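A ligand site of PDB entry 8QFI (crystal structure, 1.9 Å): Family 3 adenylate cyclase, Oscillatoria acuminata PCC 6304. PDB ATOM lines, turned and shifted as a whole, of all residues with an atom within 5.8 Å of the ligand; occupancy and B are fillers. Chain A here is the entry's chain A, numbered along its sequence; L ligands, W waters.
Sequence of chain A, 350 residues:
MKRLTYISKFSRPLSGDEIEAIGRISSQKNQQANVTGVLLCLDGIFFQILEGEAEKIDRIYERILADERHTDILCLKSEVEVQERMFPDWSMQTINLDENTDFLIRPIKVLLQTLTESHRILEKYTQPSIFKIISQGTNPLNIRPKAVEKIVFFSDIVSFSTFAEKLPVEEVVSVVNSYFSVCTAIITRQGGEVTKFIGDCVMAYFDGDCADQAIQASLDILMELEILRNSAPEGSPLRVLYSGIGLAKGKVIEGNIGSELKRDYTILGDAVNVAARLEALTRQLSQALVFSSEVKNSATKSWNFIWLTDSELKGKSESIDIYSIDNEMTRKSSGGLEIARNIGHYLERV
The side-chain amide oxygen of Asn 30 sits at hydrogen-bond distance from a nitrogen (N2) of the ligand, at 3.1 Å. O2 of the ligand sits close to OE1 of Gln 48, at 2.9 Å. O3 of the ligand lies within hydrogen-bond range of OD2 of Asp 67 (2.8 Å). An oxygen (O7) of the ligand lies within salt-bridge range of the side-chain amino group (NZ) of Lys 29, at 3.4 Å. A nitrogen (N1) of the ligand sits close to the side-chain hydroxyl of Ser 26.
The guanidinium group (NH2) of Arg 69 is in salt-bridge range of the side-chain carboxylate (OD2) of Asp 67, 3.0 Å away. The side-chain hydroxyl of Ser 26 is in hydrogen-bond range of the backbone carbonyl oxygen of Ile 22, at 2.7 Å. N of Phe 46 sits at hydrogen-bond distance from O of Ser 8 (2.8 Å). A ring nitrogen (ND1) of His 70 is in hydrogen-bond range of the side-chain hydroxyl of Ser 8, at 2.7 Å. The backbone carbonyl oxygen (O) of Ile 64 is in hydrogen-bond range of a ring nitrogen (NE2) of His 70, at 2.9 Å. The side-chain amide oxygen (OE1) of Gln 48 sits close to the side-chain sulfur (SD) of Met 92 (3.1 Å). OH of Tyr 6 is in hydrogen-bond range of NE2 of Gln 48.
Merely in contact with the ligand: Tyr 6, Ile 22, Ile 25, Phe 46, Leu 50, Ile 60, Arg 63, Ile 64, His 70 and Met 92. Hydrophobic or aromatic side chains within 4 Å of the ligand: Ile 22, Ile 25, Phe 46, Leu 50, Ile 60, Ile 64, His 70 and Met 92.
Water W1 lies within hydrogen-bond range of the backbone carbonyl oxygen of Arg 63, an oxygen (O3) of the ligand and the backbone NH of Asp 67.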
ATOM      1  N   TYR A   6      19.543  -4.132   3.950  1.00  0.00           N
ATOM      2  CA  TYR A   6      18.527  -5.055   3.454  1.00  0.00           C
ATOM      3  C   TYR A   6      18.025  -5.901   4.617  1.00  0.00           C
ATOM      4  O   TYR A   6      18.557  -5.865   5.724  1.00  0.00           O
ATOM      5  CB  TYR A   6      19.078  -5.908   2.276  1.00  0.00           C
ATOM      6  CG  TYR A   6      19.904  -7.086   2.702  1.00  0.00           C
ATOM      7  CD1 TYR A   6      19.284  -8.253   3.195  1.00  0.00           C
ATOM      8  CD2 TYR A   6      21.301  -7.042   2.627  1.00  0.00           C
ATOM      9  CE1 TYR A   6      20.047  -9.343   3.655  1.00  0.00           C
ATOM     10  CE2 TYR A   6      22.083  -8.123   3.056  1.00  0.00           C
ATOM     11  CZ  TYR A   6      21.442  -9.271   3.582  1.00  0.00           C
ATOM     12  OH  TYR A   6      22.163 -10.352   3.984  1.00  0.00           O
ATOM     13  N   SER A   8      15.839  -9.916   5.256  1.00  0.00           N
ATOM     14  CA  SER A   8      15.431 -11.157   4.635  1.00  0.00           C
ATOM     15  C   SER A   8      14.828 -12.042   5.700  1.00  0.00           C
ATOM     16  O   SER A   8      14.906 -11.758   6.898  1.00  0.00           O
ATOM     17  CB  SER A   8      16.598 -11.851   3.934  1.00  0.00           C
ATOM     18  OG  SER A   8      17.570 -12.264   4.861  1.00  0.00           O
ATOM     19  N   ILE A  22      27.963 -18.203   9.817  1.00  0.00           N
ATOM     20  CA  ILE A  22      27.824 -17.221   8.746  1.00  0.00           C
ATOM     21  C   ILE A  22      28.646 -15.974   9.067  1.00  0.00           C
ATOM     22  O   ILE A  22      29.399 -15.467   8.216  1.00  0.00           O
ATOM     23  CB  ILE A  22      26.335 -16.880   8.542  1.00  0.00           C
ATOM     24  CG1 ILE A  22      25.590 -18.076   7.928  1.00  0.00           C
ATOM     25  CG2 ILE A  22      26.150 -15.669   7.615  1.00  0.00           C
ATOM     26  CD1 ILE A  22      24.091 -18.087   8.202  1.00  0.00           C
ATOM     27  N   ILE A  25      32.630 -16.678   8.619  1.00  0.00           N
ATOM     28  CA  ILE A  25      33.023 -16.663   7.214  1.00  0.00           C
ATOM     29  C   ILE A  25      32.837 -15.267   6.615  1.00  0.00           C
ATOM     30  O   ILE A  25      33.687 -14.797   5.838  1.00  0.00           O
ATOM     31  CB  ILE A  25      32.225 -17.729   6.437  1.00  0.00           C
ATOM     32  CG1 ILE A  25      32.766 -19.124   6.774  1.00  0.00           C
ATOM     33  CG2 ILE A  25      32.290 -17.484   4.930  1.00  0.00           C
ATOM     34  CD1 ILE A  25      31.705 -20.153   7.222  1.00  0.00           C
ATOM     35  N   SER A  26      31.715 -14.601   6.914  1.00  0.00           N
ATOM     36  CA  SER A  26      31.486 -13.243   6.433  1.00  0.00           C
ATOM     37  C   SER A  26      32.576 -12.297   6.919  1.00  0.00           C
ATOM     38  O   SER A  26      33.040 -11.423   6.165  1.00  0.00           O
ATOM     39  CB  SER A  26      30.110 -12.753   6.897  1.00  0.00           C
ATOM     40  OG  SER A  26      29.080 -13.535   6.325  1.00  0.00           O
ATOM     41  N   SER A  27      32.997 -12.438   8.172  1.00  0.00           N
ATOM     42  CA  SER A  27      34.076 -11.592   8.677  1.00  0.00           C
ATOM     43  C   SER A  27      35.372 -11.823   7.892  1.00  0.00           C
ATOM     44  O   SER A  27      36.033 -10.860   7.489  1.00  0.00           O
ATOM     45  CB  SER A  27      34.284 -11.856  10.168  1.00  0.00           C
ATOM     46  OG  SER A  27      35.091 -10.840  10.748  1.00  0.00           O
ATOM     47  N   LYS A  29      35.898 -12.983   4.825  1.00  0.00           N
ATOM     48  CA  LYS A  29      35.856 -12.522   3.435  1.00  0.00           C
ATOM     49  C   LYS A  29      35.750 -11.003   3.346  1.00  0.00           C
ATOM     50  O   LYS A  29      36.291 -10.390   2.406  1.00  0.00           O
ATOM     51  CB  LYS A  29      34.708 -13.197   2.677  1.00  0.00           C
ATOM     52  CG  LYS A  29      34.814 -14.693   2.619  1.00  0.00           C
ATOM     53  CD  LYS A  29      33.638 -15.321   1.888  1.00  0.00           C
ATOM     54  CE  LYS A  29      33.667 -15.001   0.402  1.00  0.00           C
ATOM     55  NZ  LYS A  29      35.006 -15.270  -0.209  1.00  0.00           N
ATOM     56  N   ASN A  30      35.087 -10.374   4.320  1.00  0.00           N
ATOM     57  CA  ASN A  30      34.965  -8.924   4.322  1.00  0.00           C
ATOM     58  C   ASN A  30      36.244  -8.247   4.791  1.00  0.00           C
ATOM     59  O   ASN A  30      36.501  -7.097   4.378  1.00  0.00           O
ATOM     60  CB  ASN A  30      33.801  -8.512   5.211  1.00  0.00           C
ATOM     61  CG  ASN A  30      32.451  -8.730   4.529  1.00  0.00           C
ATOM     62  OD1 ASN A  30      32.363  -9.182   3.398  1.00  0.00           O
ATOM     63  ND2 ASN A  30      31.381  -8.402   5.237  1.00  0.00           N
ATOM     64  N   LEU A  39      25.534  -7.551  11.038  1.00  0.00           N
ATOM     65  CA  LEU A  39      24.525  -8.565  10.745  1.00  0.00           C
ATOM     66  C   LEU A  39      23.724  -8.768  12.011  1.00  0.00           C
ATOM     67  O   LEU A  39      24.294  -9.110  13.057  1.00  0.00           O
ATOM     68  CB  LEU A  39      25.169  -9.882  10.297  1.00  0.00           C
ATOM     69  CG  LEU A  39      24.209 -11.106  10.207  1.00  0.00           C
ATOM     70  CD1 LEU A  39      23.130 -10.882   9.194  1.00  0.00           C
ATOM     71  CD2 LEU A  39      25.021 -12.376   9.880  1.00  0.00           C
ATOM     72  N   PHE A  46      16.606 -11.541   9.143  1.00  0.00           N
ATOM     73  CA  PHE A  46      17.964 -11.021   9.041  1.00  0.00           C
ATOM     74  C   PHE A  46      17.926  -9.533   8.715  1.00  0.00           C
ATOM     75  O   PHE A  46      17.096  -9.068   7.932  1.00  0.00           O
ATOM     76  CB  PHE A  46      18.751 -11.751   7.939  1.00  0.00           C
ATOM     77  CG  PHE A  46      19.365 -13.063   8.347  1.00  0.00           C
ATOM     78  CD1 PHE A  46      20.191 -13.137   9.444  1.00  0.00           C
ATOM     79  CD2 PHE A  46      19.111 -14.234   7.606  1.00  0.00           C
ATOM     80  CE1 PHE A  46      20.754 -14.341   9.795  1.00  0.00           C
ATOM     81  CE2 PHE A  46      19.696 -15.449   7.937  1.00  0.00           C
ATOM     82  CZ  PHE A  46      20.526 -15.502   9.031  1.00  0.00           C
ATOM     83  N   GLN A  48      21.071  -6.614   7.664  1.00  0.00           N
ATOM     84  CA  GLN A  48      22.494  -6.391   7.466  1.00  0.00           C
ATOM     85  C   GLN A  48      22.746  -5.041   6.812  1.00  0.00           C
ATOM     86  O   GLN A  48      22.025  -4.628   5.902  1.00  0.00           O
ATOM     87  CB  GLN A  48      23.120  -7.466   6.575  1.00  0.00           C
ATOM     88  CG  GLN A  48      24.607  -7.224   6.227  1.00  0.00           C
ATOM     89  CD  GLN A  48      25.316  -8.485   5.817  1.00  0.00           C
ATOM     90  OE1 GLN A  48      26.424  -8.756   6.282  1.00  0.00           O
ATOM     91  NE2 GLN A  48      24.678  -9.305   4.935  1.00  0.00           N
ATOM     92  N   LEU A  50      25.985  -3.037   4.853  1.00  0.00           N
ATOM     93  CA  LEU A  50      27.212  -3.382   4.139  1.00  0.00           C
ATOM     94  C   LEU A  50      27.731  -2.141   3.443  1.00  0.00           C
ATOM     95  O   LEU A  50      27.001  -1.504   2.684  1.00  0.00           O
ATOM     96  CB  LEU A  50      26.952  -4.484   3.110  1.00  0.00           C
ATOM     97  CG  LEU A  50      27.549  -5.844   3.385  1.00  0.00           C
ATOM     98  CD1 LEU A  50      27.025  -6.843   2.368  1.00  0.00           C
ATOM     99  CD2 LEU A  50      29.053  -5.805   3.335  1.00  0.00           C
ATOM    100  N   ILE A  60      29.663  -8.851  -3.396  1.00  0.00           N
ATOM    101  CA  ILE A  60      29.248  -9.556  -2.184  1.00  0.00           C
ATOM    102  C   ILE A  60      27.722  -9.714  -2.160  1.00  0.00           C
ATOM    103  O   ILE A  60      27.206 -10.784  -1.796  1.00  0.00           O
ATOM    104  CB  ILE A  60      29.774  -8.822  -0.925  1.00  0.00           C
ATOM    105  CG1 ILE A  60      31.267  -9.126  -0.723  1.00  0.00           C
ATOM    106  CG2 ILE A  60      28.991  -9.250   0.317  1.00  0.00           C
ATOM    107  CD1 ILE A  60      32.115  -7.964  -0.403  1.00  0.00           C
ATOM    108  N   ARG A  63      26.190 -12.334  -4.444  1.00  0.00           N
ATOM    109  CA  ARG A  63      26.450 -13.654  -3.881  1.00  0.00           C
ATOM    110  C   ARG A  63      25.554 -13.956  -2.669  1.00  0.00           C
ATOM    111  O   ARG A  63      25.196 -15.125  -2.435  1.00  0.00           O
ATOM    112  CB  ARG A  63      27.928 -13.753  -3.472  1.00  0.00           C
ATOM    113  CG  ARG A  63      28.347 -15.148  -2.973  1.00  0.00           C
ATOM    114  CD  ARG A  63      28.395 -16.140  -4.124  1.00  0.00           C
ATOM    115  NE  ARG A  63      29.386 -15.777  -5.138  1.00  0.00           N
ATOM    116  CZ  ARG A  63      29.588 -16.455  -6.253  1.00  0.00           C
ATOM    117  NH1 ARG A  63      28.886 -17.536  -6.539  1.00  0.00           N
ATOM    118  NH2 ARG A  63      30.538 -16.048  -7.094  1.00  0.00           N
ATOM    119  N   ILE A  64      25.202 -12.942  -1.890  1.00  0.00           N
ATOM    120  CA  ILE A  64      24.305 -13.140  -0.753  1.00  0.00           C
ATOM    121  C   ILE A  64      22.927 -13.558  -1.231  1.00  0.00           C
ATOM    122  O   ILE A  64      22.261 -14.387  -0.616  1.00  0.00           O
ATOM    123  CB  ILE A  64      24.237 -11.874   0.104  1.00  0.00           C
ATOM    124  CG1 ILE A  64      25.539 -11.701   0.909  1.00  0.00           C
ATOM    125  CG2 ILE A  64      23.082 -11.940   1.048  1.00  0.00           C
ATOM    126  CD1 ILE A  64      25.712 -10.335   1.569  1.00  0.00           C
ATOM    127  N   LEU A  65      22.491 -13.007  -2.362  1.00  0.00           N
ATOM    128  CA  LEU A  65      21.202 -13.447  -2.892  1.00  0.00           C
ATOM    129  C   LEU A  65      21.226 -14.907  -3.316  1.00  0.00           C
ATOM    130  O   LEU A  65      20.166 -15.562  -3.363  1.00  0.00           O
ATOM    131  CB  LEU A  65      20.799 -12.593  -4.081  1.00  0.00           C
ATOM    132  CG  LEU A  65      21.111 -11.111  -4.141  1.00  0.00           C
ATOM    133  CD1 LEU A  65      21.100 -10.637  -5.612  1.00  0.00           C
ATOM    134  CD2 LEU A  65      20.088 -10.307  -3.310  1.00  0.00           C
ATOM    135  N   ALA A  66      22.406 -15.443  -3.622  1.00  0.00           N
ATOM    136  CA  ALA A  66      22.548 -16.855  -3.962  1.00  0.00           C
ATOM    137  C   ALA A  66      22.415 -17.757  -2.740  1.00  0.00           C
ATOM    138  O   ALA A  66      22.152 -18.944  -2.926  1.00  0.00           O
ATOM    139  CB  ALA A  66      23.889 -17.119  -4.655  1.00  0.00           C
ATOM    140  N   ASP A  67      22.595 -17.215  -1.528  1.00  0.00           N
ATOM    141  CA  ASP A  67      22.551 -18.035  -0.316  1.00  0.00           C
ATOM    142  C   ASP A  67      21.144 -18.606  -0.105  1.00  0.00           C
ATOM    143  O   ASP A  67      20.156 -17.874  -0.096  1.00  0.00           O
ATOM    144  CB  ASP A  67      22.959 -17.217   0.905  1.00  0.00           C
ATOM    145  CG  ASP A  67      23.605 -18.070   1.984  1.00  0.00           C
ATOM    146  OD1 ASP A  67      22.890 -18.899   2.588  1.00  0.00           O
ATOM    147  OD2 ASP A  67      24.828 -17.890   2.230  1.00  0.00           O
ATOM    148  N   ARG A  69      19.995 -20.082   2.626  1.00  0.00           N
ATOM    149  CA  ARG A  69      19.500 -20.085   4.002  1.00  0.00           C
ATOM    150  C   ARG A  69      18.602 -18.887   4.310  1.00  0.00           C
ATOM    151  O   ARG A  69      18.101 -18.823   5.440  1.00  0.00           O
ATOM    152  CB  ARG A  69      20.672 -20.112   4.981  1.00  0.00           C
ATOM    153  CG  ARG A  69      21.315 -21.488   5.094  1.00  0.00           C
ATOM    154  CD  ARG A  69      22.686 -21.416   5.752  1.00  0.00           C
ATOM    155  NE  ARG A  69      23.636 -20.677   4.936  1.00  0.00           N
ATOM    156  CZ  ARG A  69      24.870 -20.372   5.324  1.00  0.00           C
ATOM    157  NH1 ARG A  69      25.333 -20.741   6.504  1.00  0.00           N
ATOM    158  NH2 ARG A  69      25.648 -19.661   4.512  1.00  0.00           N
ATOM    159  N   HIS A  70      18.399 -17.959   3.375  1.00  0.00           N
ATOM    160  CA  HIS A  70      17.463 -16.854   3.566  1.00  0.00           C
ATOM    161  C   HIS A  70      16.777 -16.547   2.246  1.00  0.00           C
ATOM    162  O   HIS A  70      17.264 -16.855   1.159  1.00  0.00           O
ATOM    163  CB  HIS A  70      18.156 -15.615   4.147  1.00  0.00           C
ATOM    164  CG  HIS A  70      19.076 -14.918   3.195  1.00  0.00           C
ATOM    165  ND1 HIS A  70      19.434 -13.590   3.343  1.00  0.00           N
ATOM    166  CD2 HIS A  70      19.711 -15.354   2.080  1.00  0.00           C
ATOM    167  CE1 HIS A  70      20.237 -13.242   2.361  1.00  0.00           C
ATOM    168  NE2 HIS A  70      20.421 -14.290   1.583  1.00  0.00           N
ATOM    169  N   MET A  92      32.544  -7.803   9.993  1.00  0.00           N
ATOM    170  CA  MET A  92      31.186  -8.339  10.136  1.00  0.00           C
ATOM    171  C   MET A  92      30.956  -8.567  11.616  1.00  0.00           C
ATOM    172  O   MET A  92      31.555  -9.486  12.187  1.00  0.00           O
ATOM    173  CB  MET A  92      31.014  -9.626   9.357  1.00  0.00           C
ATOM    174  CG  MET A  92      29.671 -10.296   9.588  1.00  0.00           C
ATOM    175  SD  MET A  92      28.413  -9.701   8.453  1.00  0.00           S
ATOM    176  CE  MET A  92      27.979  -8.159   9.150  1.00  0.00           C
HETATM  177  N1  LIG L   1      29.395 -13.555   2.860  1.00  0.00           N
HETATM  178  C1  LIG L   1      30.357 -12.429   2.824  1.00  0.00           C
HETATM  179  O1  LIG L   1      31.436 -12.531   2.343  1.00  0.00           O
HETATM  180  N2  LIG L   1      29.997 -11.126   3.420  1.00  0.00           N
HETATM  181  C2  LIG L   1      28.702 -10.955   4.028  1.00  0.00           C
HETATM  182  O2  LIG L   1      28.443  -9.896   4.498  1.00  0.00           O
HETATM  183  C3  LIG L   1      27.706 -12.100   4.013  1.00  0.00           C
HETATM  184  N3  LIG L   1      26.415 -11.927   4.604  1.00  0.00           N
HETATM  185  C4  LIG L   1      25.423 -13.033   4.640  1.00  0.00           C
HETATM  186  C5  LIG L   1      24.154 -12.823   5.227  1.00  0.00           C
HETATM  187  C6  LIG L   1      23.234 -13.876   5.255  1.00  0.00           C
HETATM  188  C7  LIG L   1      22.002 -13.304   5.943  1.00  0.00           C
HETATM  189  C8  LIG L   1      23.576 -15.131   4.676  1.00  0.00           C
HETATM  190  C9  LIG L   1      22.507 -16.228   4.755  1.00  0.00           C
HETATM  191  C10 LIG L   1      24.842 -15.328   4.107  1.00  0.00           C
HETATM  192  C11 LIG L   1      25.782 -14.272   4.061  1.00  0.00           C
HETATM  193  N4  LIG L   1      27.142 -14.443   3.462  1.00  0.00           N
HETATM  194  C12 LIG L   1      28.071 -13.360   3.427  1.00  0.00           C
HETATM  195  C13 LIG L   1      27.525 -15.727   2.926  1.00  0.00           C
HETATM  196  C14 LIG L   1      27.559 -15.725   1.425  1.00  0.00           C
HETATM  197  O3  LIG L   1      26.234 -15.774   0.981  1.00  0.00           O
HETATM  198  C15 LIG L   1      28.289 -16.962   0.890  1.00  0.00           C
HETATM  199  O4  LIG L   1      27.836 -18.133   1.529  1.00  0.00           O
HETATM  200  C16 LIG L   1      29.790 -16.850   1.113  1.00  0.00           C
HETATM  201  O5  LIG L   1      30.263 -15.638   0.618  1.00  0.00           O
HETATM  202  C17 LIG L   1      30.483 -18.018   0.373  1.00  0.00           C
HETATM  203  O6  LIG L   1      31.456 -18.563   1.255  1.00  0.00           O
HETATM  204  P1  LIG L   1      32.743 -19.422   0.641  1.00  0.00           P
HETATM  205  O7  LIG L   1      33.886 -18.439   0.399  1.00  0.00           O
HETATM  206  O8  LIG L   1      33.182 -20.455   1.671  1.00  0.00           O
HETATM  207  O9  LIG L   1      32.272 -20.059  -0.664  1.00  0.00           O
HETATM  208  O   HOH W   1      25.817 -17.704  -1.532  1.00  0.00           O
